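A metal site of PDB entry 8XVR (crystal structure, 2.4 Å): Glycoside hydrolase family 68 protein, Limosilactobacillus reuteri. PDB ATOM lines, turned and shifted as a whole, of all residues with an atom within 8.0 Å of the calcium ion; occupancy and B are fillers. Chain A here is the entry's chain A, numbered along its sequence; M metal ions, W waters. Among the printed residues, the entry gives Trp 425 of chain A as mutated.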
ATOM      1  N   GLN A 286      12.901  -2.323 -21.844  1.00  0.00           N
ATOM      2  CA  GLN A 286      13.004  -2.515 -23.284  1.00  0.00           C
ATOM      3  C   GLN A 286      12.215  -1.441 -24.073  1.00  0.00           C
ATOM      4  O   GLN A 286      11.097  -1.083 -23.717  1.00  0.00           O
ATOM      5  CB  GLN A 286      12.519  -3.917 -23.664  1.00  0.00           C
ATOM      6  CG  GLN A 286      12.860  -4.318 -25.072  1.00  0.00           C
ATOM      7  CD  GLN A 286      12.123  -5.571 -25.549  1.00  0.00           C
ATOM      8  OE1 GLN A 286      10.913  -5.689 -25.422  1.00  0.00           O
ATOM      9  NE2 GLN A 286      12.862  -6.488 -26.147  1.00  0.00           N
ATOM     10  N   TRP A 291      12.997  -3.973 -29.391  1.00  0.00           N
ATOM     11  CA  TRP A 291      12.127  -5.123 -29.657  1.00  0.00           C
ATOM     12  C   TRP A 291      12.088  -5.392 -31.163  1.00  0.00           C
ATOM     13  O   TRP A 291      12.216  -6.541 -31.605  1.00  0.00           O
ATOM     14  CB  TRP A 291      10.722  -4.897 -29.091  1.00  0.00           C
ATOM     15  CG  TRP A 291       9.718  -5.888 -29.547  1.00  0.00           C
ATOM     16  CD1 TRP A 291       9.486  -7.151 -29.028  1.00  0.00           C
ATOM     17  CD2 TRP A 291       8.802  -5.732 -30.624  1.00  0.00           C
ATOM     18  NE1 TRP A 291       8.486  -7.785 -29.731  1.00  0.00           N
ATOM     19  CE2 TRP A 291       8.049  -6.934 -30.722  1.00  0.00           C
ATOM     20  CE3 TRP A 291       8.560  -4.693 -31.534  1.00  0.00           C
ATOM     21  CZ2 TRP A 291       7.032  -7.097 -31.701  1.00  0.00           C
ATOM     22  CZ3 TRP A 291       7.578  -4.854 -32.486  1.00  0.00           C
ATOM     23  CH2 TRP A 291       6.821  -6.069 -32.564  1.00  0.00           C
ATOM     24  N   ALA A 298       9.147 -14.416 -31.827  1.00  0.00           N
ATOM     25  CA  ALA A 298       9.121 -15.085 -30.514  1.00  0.00           C
ATOM     26  C   ALA A 298       9.090 -14.114 -29.285  1.00  0.00           C
ATOM     27  O   ALA A 298       8.927 -14.578 -28.146  1.00  0.00           O
ATOM     28  CB  ALA A 298      10.336 -16.039 -30.399  1.00  0.00           C
ATOM     29  N   ASP A 299       9.269 -12.799 -29.507  1.00  0.00           N
ATOM     30  CA  ASP A 299       9.434 -11.836 -28.404  1.00  0.00           C
ATOM     31  C   ASP A 299       8.185 -11.017 -28.111  1.00  0.00           C
ATOM     32  O   ASP A 299       7.583 -10.433 -29.005  1.00  0.00           O
ATOM     33  CB  ASP A 299      10.597 -10.867 -28.675  1.00  0.00           C
ATOM     34  CG  ASP A 299      11.153 -10.226 -27.376  1.00  0.00           C
ATOM     35  OD1 ASP A 299      10.863 -10.753 -26.268  1.00  0.00           O
ATOM     36  OD2 ASP A 299      11.877  -9.205 -27.469  1.00  0.00           O
ATOM     37  N   ASN A 300       7.813 -10.932 -26.843  1.00  0.00           N
ATOM     38  CA  ASN A 300       6.671 -10.092 -26.457  1.00  0.00           C
ATOM     39  C   ASN A 300       7.094  -8.646 -26.455  1.00  0.00           C
ATOM     40  O   ASN A 300       8.301  -8.328 -26.353  1.00  0.00           O
ATOM     41  CB  ASN A 300       6.162 -10.481 -25.066  1.00  0.00           C
ATOM     42  CG  ASN A 300       4.722 -10.077 -24.837  1.00  0.00           C
ATOM     43  OD1 ASN A 300       4.021  -9.703 -25.755  1.00  0.00           O
ATOM     44  ND2 ASN A 300       4.280 -10.170 -23.594  1.00  0.00           N
ATOM     45  N   ILE A 301       6.124  -7.774 -26.539  1.00  0.00           N
ATOM     46  CA  ILE A 301       6.380  -6.363 -26.301  1.00  0.00           C
ATOM     47  C   ILE A 301       5.384  -5.815 -25.285  1.00  0.00           C
ATOM     48  O   ILE A 301       4.169  -5.981 -25.414  1.00  0.00           O
ATOM     49  CB  ILE A 301       6.377  -5.545 -27.633  1.00  0.00           C
ATOM     50  CG1 ILE A 301       6.572  -4.084 -27.325  1.00  0.00           C
ATOM     51  CG2 ILE A 301       5.115  -5.754 -28.464  1.00  0.00           C
ATOM     52  CD1 ILE A 301       6.975  -3.257 -28.512  1.00  0.00           C
ATOM     53  N   ALA A 302       5.924  -5.145 -24.268  1.00  0.00           N
ATOM     54  CA  ALA A 302       5.156  -4.705 -23.143  1.00  0.00           C
ATOM     55  C   ALA A 302       5.660  -3.344 -22.632  1.00  0.00           C
ATOM     56  O   ALA A 302       6.836  -3.195 -22.267  1.00  0.00           O
ATOM     57  CB  ALA A 302       5.205  -5.756 -22.037  1.00  0.00           C
ATOM     58  N   ALA A 322       6.485  -4.042 -18.127  1.00  0.00           N
ATOM     59  CA  ALA A 322       7.451  -3.901 -19.167  1.00  0.00           C
ATOM     60  C   ALA A 322       8.313  -5.159 -19.320  1.00  0.00           C
ATOM     61  O   ALA A 322       8.015  -6.186 -18.758  1.00  0.00           O
ATOM     62  CB  ALA A 322       8.317  -2.678 -18.826  1.00  0.00           C
ATOM     63  N   SER A 323       9.389  -5.051 -20.078  1.00  0.00           N
ATOM     64  CA  SER A 323      10.431  -6.075 -20.125  1.00  0.00           C
ATOM     65  C   SER A 323      11.750  -5.413 -19.739  1.00  0.00           C
ATOM     66  O   SER A 323      11.882  -4.213 -19.878  1.00  0.00           O
ATOM     67  CB  SER A 323      10.468  -6.709 -21.531  1.00  0.00           C
ATOM     68  OG  SER A 323       9.171  -7.015 -22.024  1.00  0.00           O
ATOM     69  N   THR A 324      12.722  -6.162 -19.230  1.00  0.00           N
ATOM     70  CA  THR A 324      14.033  -5.589 -18.897  1.00  0.00           C
ATOM     71  C   THR A 324      14.722  -5.020 -20.128  1.00  0.00           C
ATOM     72  O   THR A 324      14.495  -5.478 -21.233  1.00  0.00           O
ATOM     73  CB  THR A 324      15.004  -6.627 -18.274  1.00  0.00           C
ATOM     74  OG1 THR A 324      15.191  -7.729 -19.193  1.00  0.00           O
ATOM     75  CG2 THR A 324      14.456  -7.154 -16.965  1.00  0.00           C
ATOM     76  N   TYR A 329      19.301  -8.159 -19.811  1.00  0.00           N
ATOM     77  CA  TYR A 329      18.479  -8.355 -21.016  1.00  0.00           C
ATOM     78  C   TYR A 329      18.212  -9.828 -21.292  1.00  0.00           C
ATOM     79  O   TYR A 329      18.971 -10.693 -20.861  1.00  0.00           O
ATOM     80  CB  TYR A 329      19.169  -7.728 -22.238  1.00  0.00           C
ATOM     81  CG  TYR A 329      18.236  -7.347 -23.389  1.00  0.00           C
ATOM     82  CD1 TYR A 329      17.015  -6.720 -23.135  1.00  0.00           C
ATOM     83  CD2 TYR A 329      18.580  -7.588 -24.733  1.00  0.00           C
ATOM     84  CE1 TYR A 329      16.166  -6.357 -24.172  1.00  0.00           C
ATOM     85  CE2 TYR A 329      17.723  -7.253 -25.764  1.00  0.00           C
ATOM     86  CZ  TYR A 329      16.516  -6.606 -25.467  1.00  0.00           C
ATOM     87  OH  TYR A 329      15.629  -6.236 -26.459  1.00  0.00           O
ATOM     88  N   GLN A 330      17.125 -10.093 -22.009  1.00  0.00           N
ATOM     89  CA  GLN A 330      16.870 -11.406 -22.562  1.00  0.00           C
ATOM     90  C   GLN A 330      18.084 -11.877 -23.361  1.00  0.00           C
ATOM     91  O   GLN A 330      18.833 -11.068 -23.890  1.00  0.00           O
ATOM     92  CB  GLN A 330      15.621 -11.364 -23.474  1.00  0.00           C
ATOM     93  CG  GLN A 330      15.764 -10.471 -24.699  1.00  0.00           C
ATOM     94  CD  GLN A 330      14.405 -10.100 -25.313  1.00  0.00           C
ATOM     95  OE1 GLN A 330      13.373 -10.173 -24.670  1.00  0.00           O
ATOM     96  NE2 GLN A 330      14.421  -9.669 -26.578  1.00  0.00           N
ATOM     97  N   GLY A 331      18.250 -13.189 -23.451  1.00  0.00           N
ATOM     98  CA  GLY A 331      19.194 -13.822 -24.383  1.00  0.00           C
ATOM     99  C   GLY A 331      19.406 -15.283 -24.022  1.00  0.00           C
ATOM    100  O   GLY A 331      19.019 -15.724 -22.939  1.00  0.00           O
ATOM    101  N   ARG A 364      11.820 -20.088 -25.489  1.00  0.00           N
ATOM    102  CA  ARG A 364      11.086 -19.237 -24.546  1.00  0.00           C
ATOM    103  C   ARG A 364      12.019 -18.663 -23.480  1.00  0.00           C
ATOM    104  O   ARG A 364      11.931 -17.491 -23.132  1.00  0.00           O
ATOM    105  CB  ARG A 364       9.955 -20.016 -23.865  1.00  0.00           C
ATOM    106  CG  ARG A 364       8.732 -20.194 -24.717  1.00  0.00           C
ATOM    107  CD  ARG A 364       7.813 -21.161 -24.057  1.00  0.00           C
ATOM    108  NE  ARG A 364       6.576 -21.370 -24.812  1.00  0.00           N
ATOM    109  CZ  ARG A 364       5.396 -20.811 -24.542  1.00  0.00           C
ATOM    110  NH1 ARG A 364       5.227 -20.011 -23.503  1.00  0.00           N
ATOM    111  NH2 ARG A 364       4.356 -21.120 -25.299  1.00  0.00           N
ATOM    112  N   ALA A 365      12.909 -19.487 -22.935  1.00  0.00           N
ATOM    113  CA  ALA A 365      13.847 -19.045 -21.924  1.00  0.00           C
ATOM    114  C   ALA A 365      14.781 -17.998 -22.468  1.00  0.00           C
ATOM    115  O   ALA A 365      15.185 -17.071 -21.743  1.00  0.00           O
ATOM    116  CB  ALA A 365      14.640 -20.224 -21.424  1.00  0.00           C
ATOM    117  N   THR A 366      15.118 -18.142 -23.744  1.00  0.00           N
ATOM    118  CA  THR A 366      15.949 -17.211 -24.493  1.00  0.00           C
ATOM    119  C   THR A 366      15.309 -15.819 -24.710  1.00  0.00           C
ATOM    120  O   THR A 366      16.033 -14.820 -24.838  1.00  0.00           O
ATOM    121  CB  THR A 366      16.337 -17.868 -25.844  1.00  0.00           C
ATOM    122  OG1 THR A 366      17.256 -18.939 -25.574  1.00  0.00           O
ATOM    123  CG2 THR A 366      16.951 -16.895 -26.832  1.00  0.00           C
ATOM    124  N   TRP A 367      13.957 -15.761 -24.735  1.00  0.00           N
ATOM    125  CA  TRP A 367      13.222 -14.524 -24.939  1.00  0.00           C
ATOM    126  C   TRP A 367      12.504 -13.942 -23.691  1.00  0.00           C
ATOM    127  O   TRP A 367      11.997 -12.849 -23.731  1.00  0.00           O
ATOM    128  CB  TRP A 367      12.234 -14.688 -26.104  1.00  0.00           C
ATOM    129  CG  TRP A 367      12.923 -14.964 -27.401  1.00  0.00           C
ATOM    130  CD1 TRP A 367      13.060 -16.178 -28.002  1.00  0.00           C
ATOM    131  CD2 TRP A 367      13.537 -14.006 -28.297  1.00  0.00           C
ATOM    132  NE1 TRP A 367      13.740 -16.050 -29.188  1.00  0.00           N
ATOM    133  CE2 TRP A 367      14.046 -14.736 -29.397  1.00  0.00           C
ATOM    134  CE3 TRP A 367      13.725 -12.610 -28.247  1.00  0.00           C
ATOM    135  CZ2 TRP A 367      14.724 -14.138 -30.456  1.00  0.00           C
ATOM    136  CZ3 TRP A 367      14.412 -12.006 -29.306  1.00  0.00           C
ATOM    137  CH2 TRP A 367      14.900 -12.781 -30.407  1.00  0.00           C
ATOM    138  N   ALA A 368      12.512 -14.664 -22.589  1.00  0.00           N
ATOM    139  CA  ALA A 368      11.776 -14.254 -21.375  1.00  0.00           C
ATOM    140  C   ALA A 368      12.532 -13.208 -20.532  1.00  0.00           C
ATOM    141  O   ALA A 368      13.668 -13.443 -20.061  1.00  0.00           O
ATOM    142  CB  ALA A 368      11.461 -15.471 -20.502  1.00  0.00           C
ATOM    143  N   ASN A 369      11.864 -12.080 -20.319  1.00  0.00           N
ATOM    144  CA  ASN A 369      12.365 -11.030 -19.425  1.00  0.00           C
ATOM    145  C   ASN A 369      11.285 -10.035 -18.986  1.00  0.00           C
ATOM    146  O   ASN A 369      11.511  -8.826 -18.975  1.00  0.00           O
ATOM    147  CB  ASN A 369      13.534 -10.296 -20.082  1.00  0.00           C
ATOM    148  CG  ASN A 369      13.117  -9.495 -21.318  1.00  0.00           C
ATOM    149  OD1 ASN A 369      12.161  -9.848 -22.047  1.00  0.00           O
ATOM    150  ND2 ASN A 369      13.828  -8.381 -21.541  1.00  0.00           N
ATOM    151  N   ALA A 370      10.140 -10.547 -18.582  1.00  0.00           N
ATOM    152  CA  ALA A 370       9.100  -9.693 -18.032  1.00  0.00           C
ATOM    153  C   ALA A 370       9.654  -8.878 -16.882  1.00  0.00           C
ATOM    154  O   ALA A 370      10.516  -9.342 -16.134  1.00  0.00           O
ATOM    155  CB  ALA A 370       7.901 -10.550 -17.583  1.00  0.00           C
ATOM    156  N   SER A 400       9.518 -15.930 -17.428  1.00  0.00           N
ATOM    157  CA  SER A 400       8.284 -15.480 -18.118  1.00  0.00           C
ATOM    158  C   SER A 400       8.503 -14.233 -18.934  1.00  0.00           C
ATOM    159  O   SER A 400       9.334 -13.408 -18.567  1.00  0.00           O
ATOM    160  CB  SER A 400       7.158 -15.188 -17.105  1.00  0.00           C
ATOM    161  OG  SER A 400       5.978 -14.849 -17.767  1.00  0.00           O
ATOM    162  N   ASP A 401       7.738 -14.079 -20.014  1.00  0.00           N
ATOM    163  CA  ASP A 401       7.725 -12.851 -20.831  1.00  0.00           C
ATOM    164  C   ASP A 401       6.387 -12.091 -20.741  1.00  0.00           C
ATOM    165  O   ASP A 401       6.148 -11.190 -21.544  1.00  0.00           O
ATOM    166  CB  ASP A 401       8.085 -13.187 -22.308  1.00  0.00           C
ATOM    167  CG  ASP A 401       8.986 -12.132 -22.977  1.00  0.00           C
ATOM    168  OD1 ASP A 401       9.789 -11.416 -22.273  1.00  0.00           O
ATOM    169  OD2 ASP A 401       8.918 -12.036 -24.245  1.00  0.00           O
ATOM    170  N   GLU A 402       5.520 -12.430 -19.787  1.00  0.00           N
ATOM    171  CA  GLU A 402       4.350 -11.588 -19.505  1.00  0.00           C
ATOM    172  C   GLU A 402       3.826 -11.629 -18.070  1.00  0.00           C
ATOM    173  O   GLU A 402       3.367 -12.702 -17.578  1.00  0.00           O
ATOM    174  CB  GLU A 402       3.187 -11.936 -20.455  1.00  0.00           C
ATOM    175  CG  GLU A 402       2.134 -10.838 -20.496  1.00  0.00           C
ATOM    176  CD  GLU A 402       1.079 -11.099 -21.533  1.00  0.00           C
ATOM    177  OE1 GLU A 402       0.061 -11.732 -21.157  1.00  0.00           O
ATOM    178  OE2 GLU A 402       1.250 -10.692 -22.717  1.00  0.00           O
ATOM    179  N   TRP A 425       2.498 -17.991 -20.681  1.00  0.00           N
ATOM    180  CA  TRP A 425       3.536 -17.078 -21.145  1.00  0.00           C
ATOM    181  C   TRP A 425       4.900 -17.379 -20.543  1.00  0.00           C
ATOM    182  O   TRP A 425       5.865 -16.643 -20.755  1.00  0.00           O
ATOM    183  CB  TRP A 425       3.150 -15.632 -20.823  1.00  0.00           C
ATOM    184  CG  TRP A 425       2.387 -15.020 -21.896  1.00  0.00           C
ATOM    185  CD1 TRP A 425       1.035 -14.867 -21.982  1.00  0.00           C
ATOM    186  CD2 TRP A 425       2.930 -14.479 -23.098  1.00  0.00           C
ATOM    187  NE1 TRP A 425       0.707 -14.257 -23.168  1.00  0.00           N
ATOM    188  CE2 TRP A 425       1.853 -14.006 -23.874  1.00  0.00           C
ATOM    189  CE3 TRP A 425       4.251 -14.397 -23.617  1.00  0.00           C
ATOM    190  CZ2 TRP A 425       2.019 -13.434 -25.122  1.00  0.00           C
ATOM    191  CZ3 TRP A 425       4.428 -13.825 -24.872  1.00  0.00           C
ATOM    192  CH2 TRP A 425       3.316 -13.350 -25.625  1.00  0.00           C
HETATM  193 CA    CA M   1      11.237 -10.673 -23.990  1.00  0.00          CA
HETATM  194  O   HOH W   1       9.789  -8.911 -24.331  1.00  0.00           O
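N of Asn 369 lies within hydrogen-bond range of O of Ser 400, 3.4 Å away.
The side-chain amide nitrogen (ND2) of Asn 369 is in hydrogen-bond range of the side-chain hydroxyl (OG1) of Thr 324 (2.8 Å).
The side-chain carboxylate of Asp 299 is in hydrogen-bond range of the side-chain amide nitrogen of Gln 286, 3.2 Å away.
O of Asp 299 is in hydrogen-bond range of NE1 of Trp 291.
The backbone carbonyl oxygen of Asp 401 is in hydrogen-bond range of the side-chain amide nitrogen of Asn 300 (3.0 Å).
N of Asp 401 lies within hydrogen-bond range of O of Trp 425 (3.3 Å).
Water W1 bridges the backbone carbonyl oxygen (O) of Asn 300 (2.6 Å) and the side-chain hydroxyl (OG) of Ser 323 (3.0 Å).
The calcium ion is bound by the side-chain amide oxygen (OE1) of Gln 330, the side-chain amide oxygen (OD1) of Asn 369, water W1, the side-chain carboxylate (OD1) of Asp 299, the backbone carbonyl oxygen (O) of Trp 367, the side-chain carboxylate (OD1) of Asp 401 and the side-chain carboxylate (OD2) of Asp 401.
The calcium ion has seven donor atoms within binding distance.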
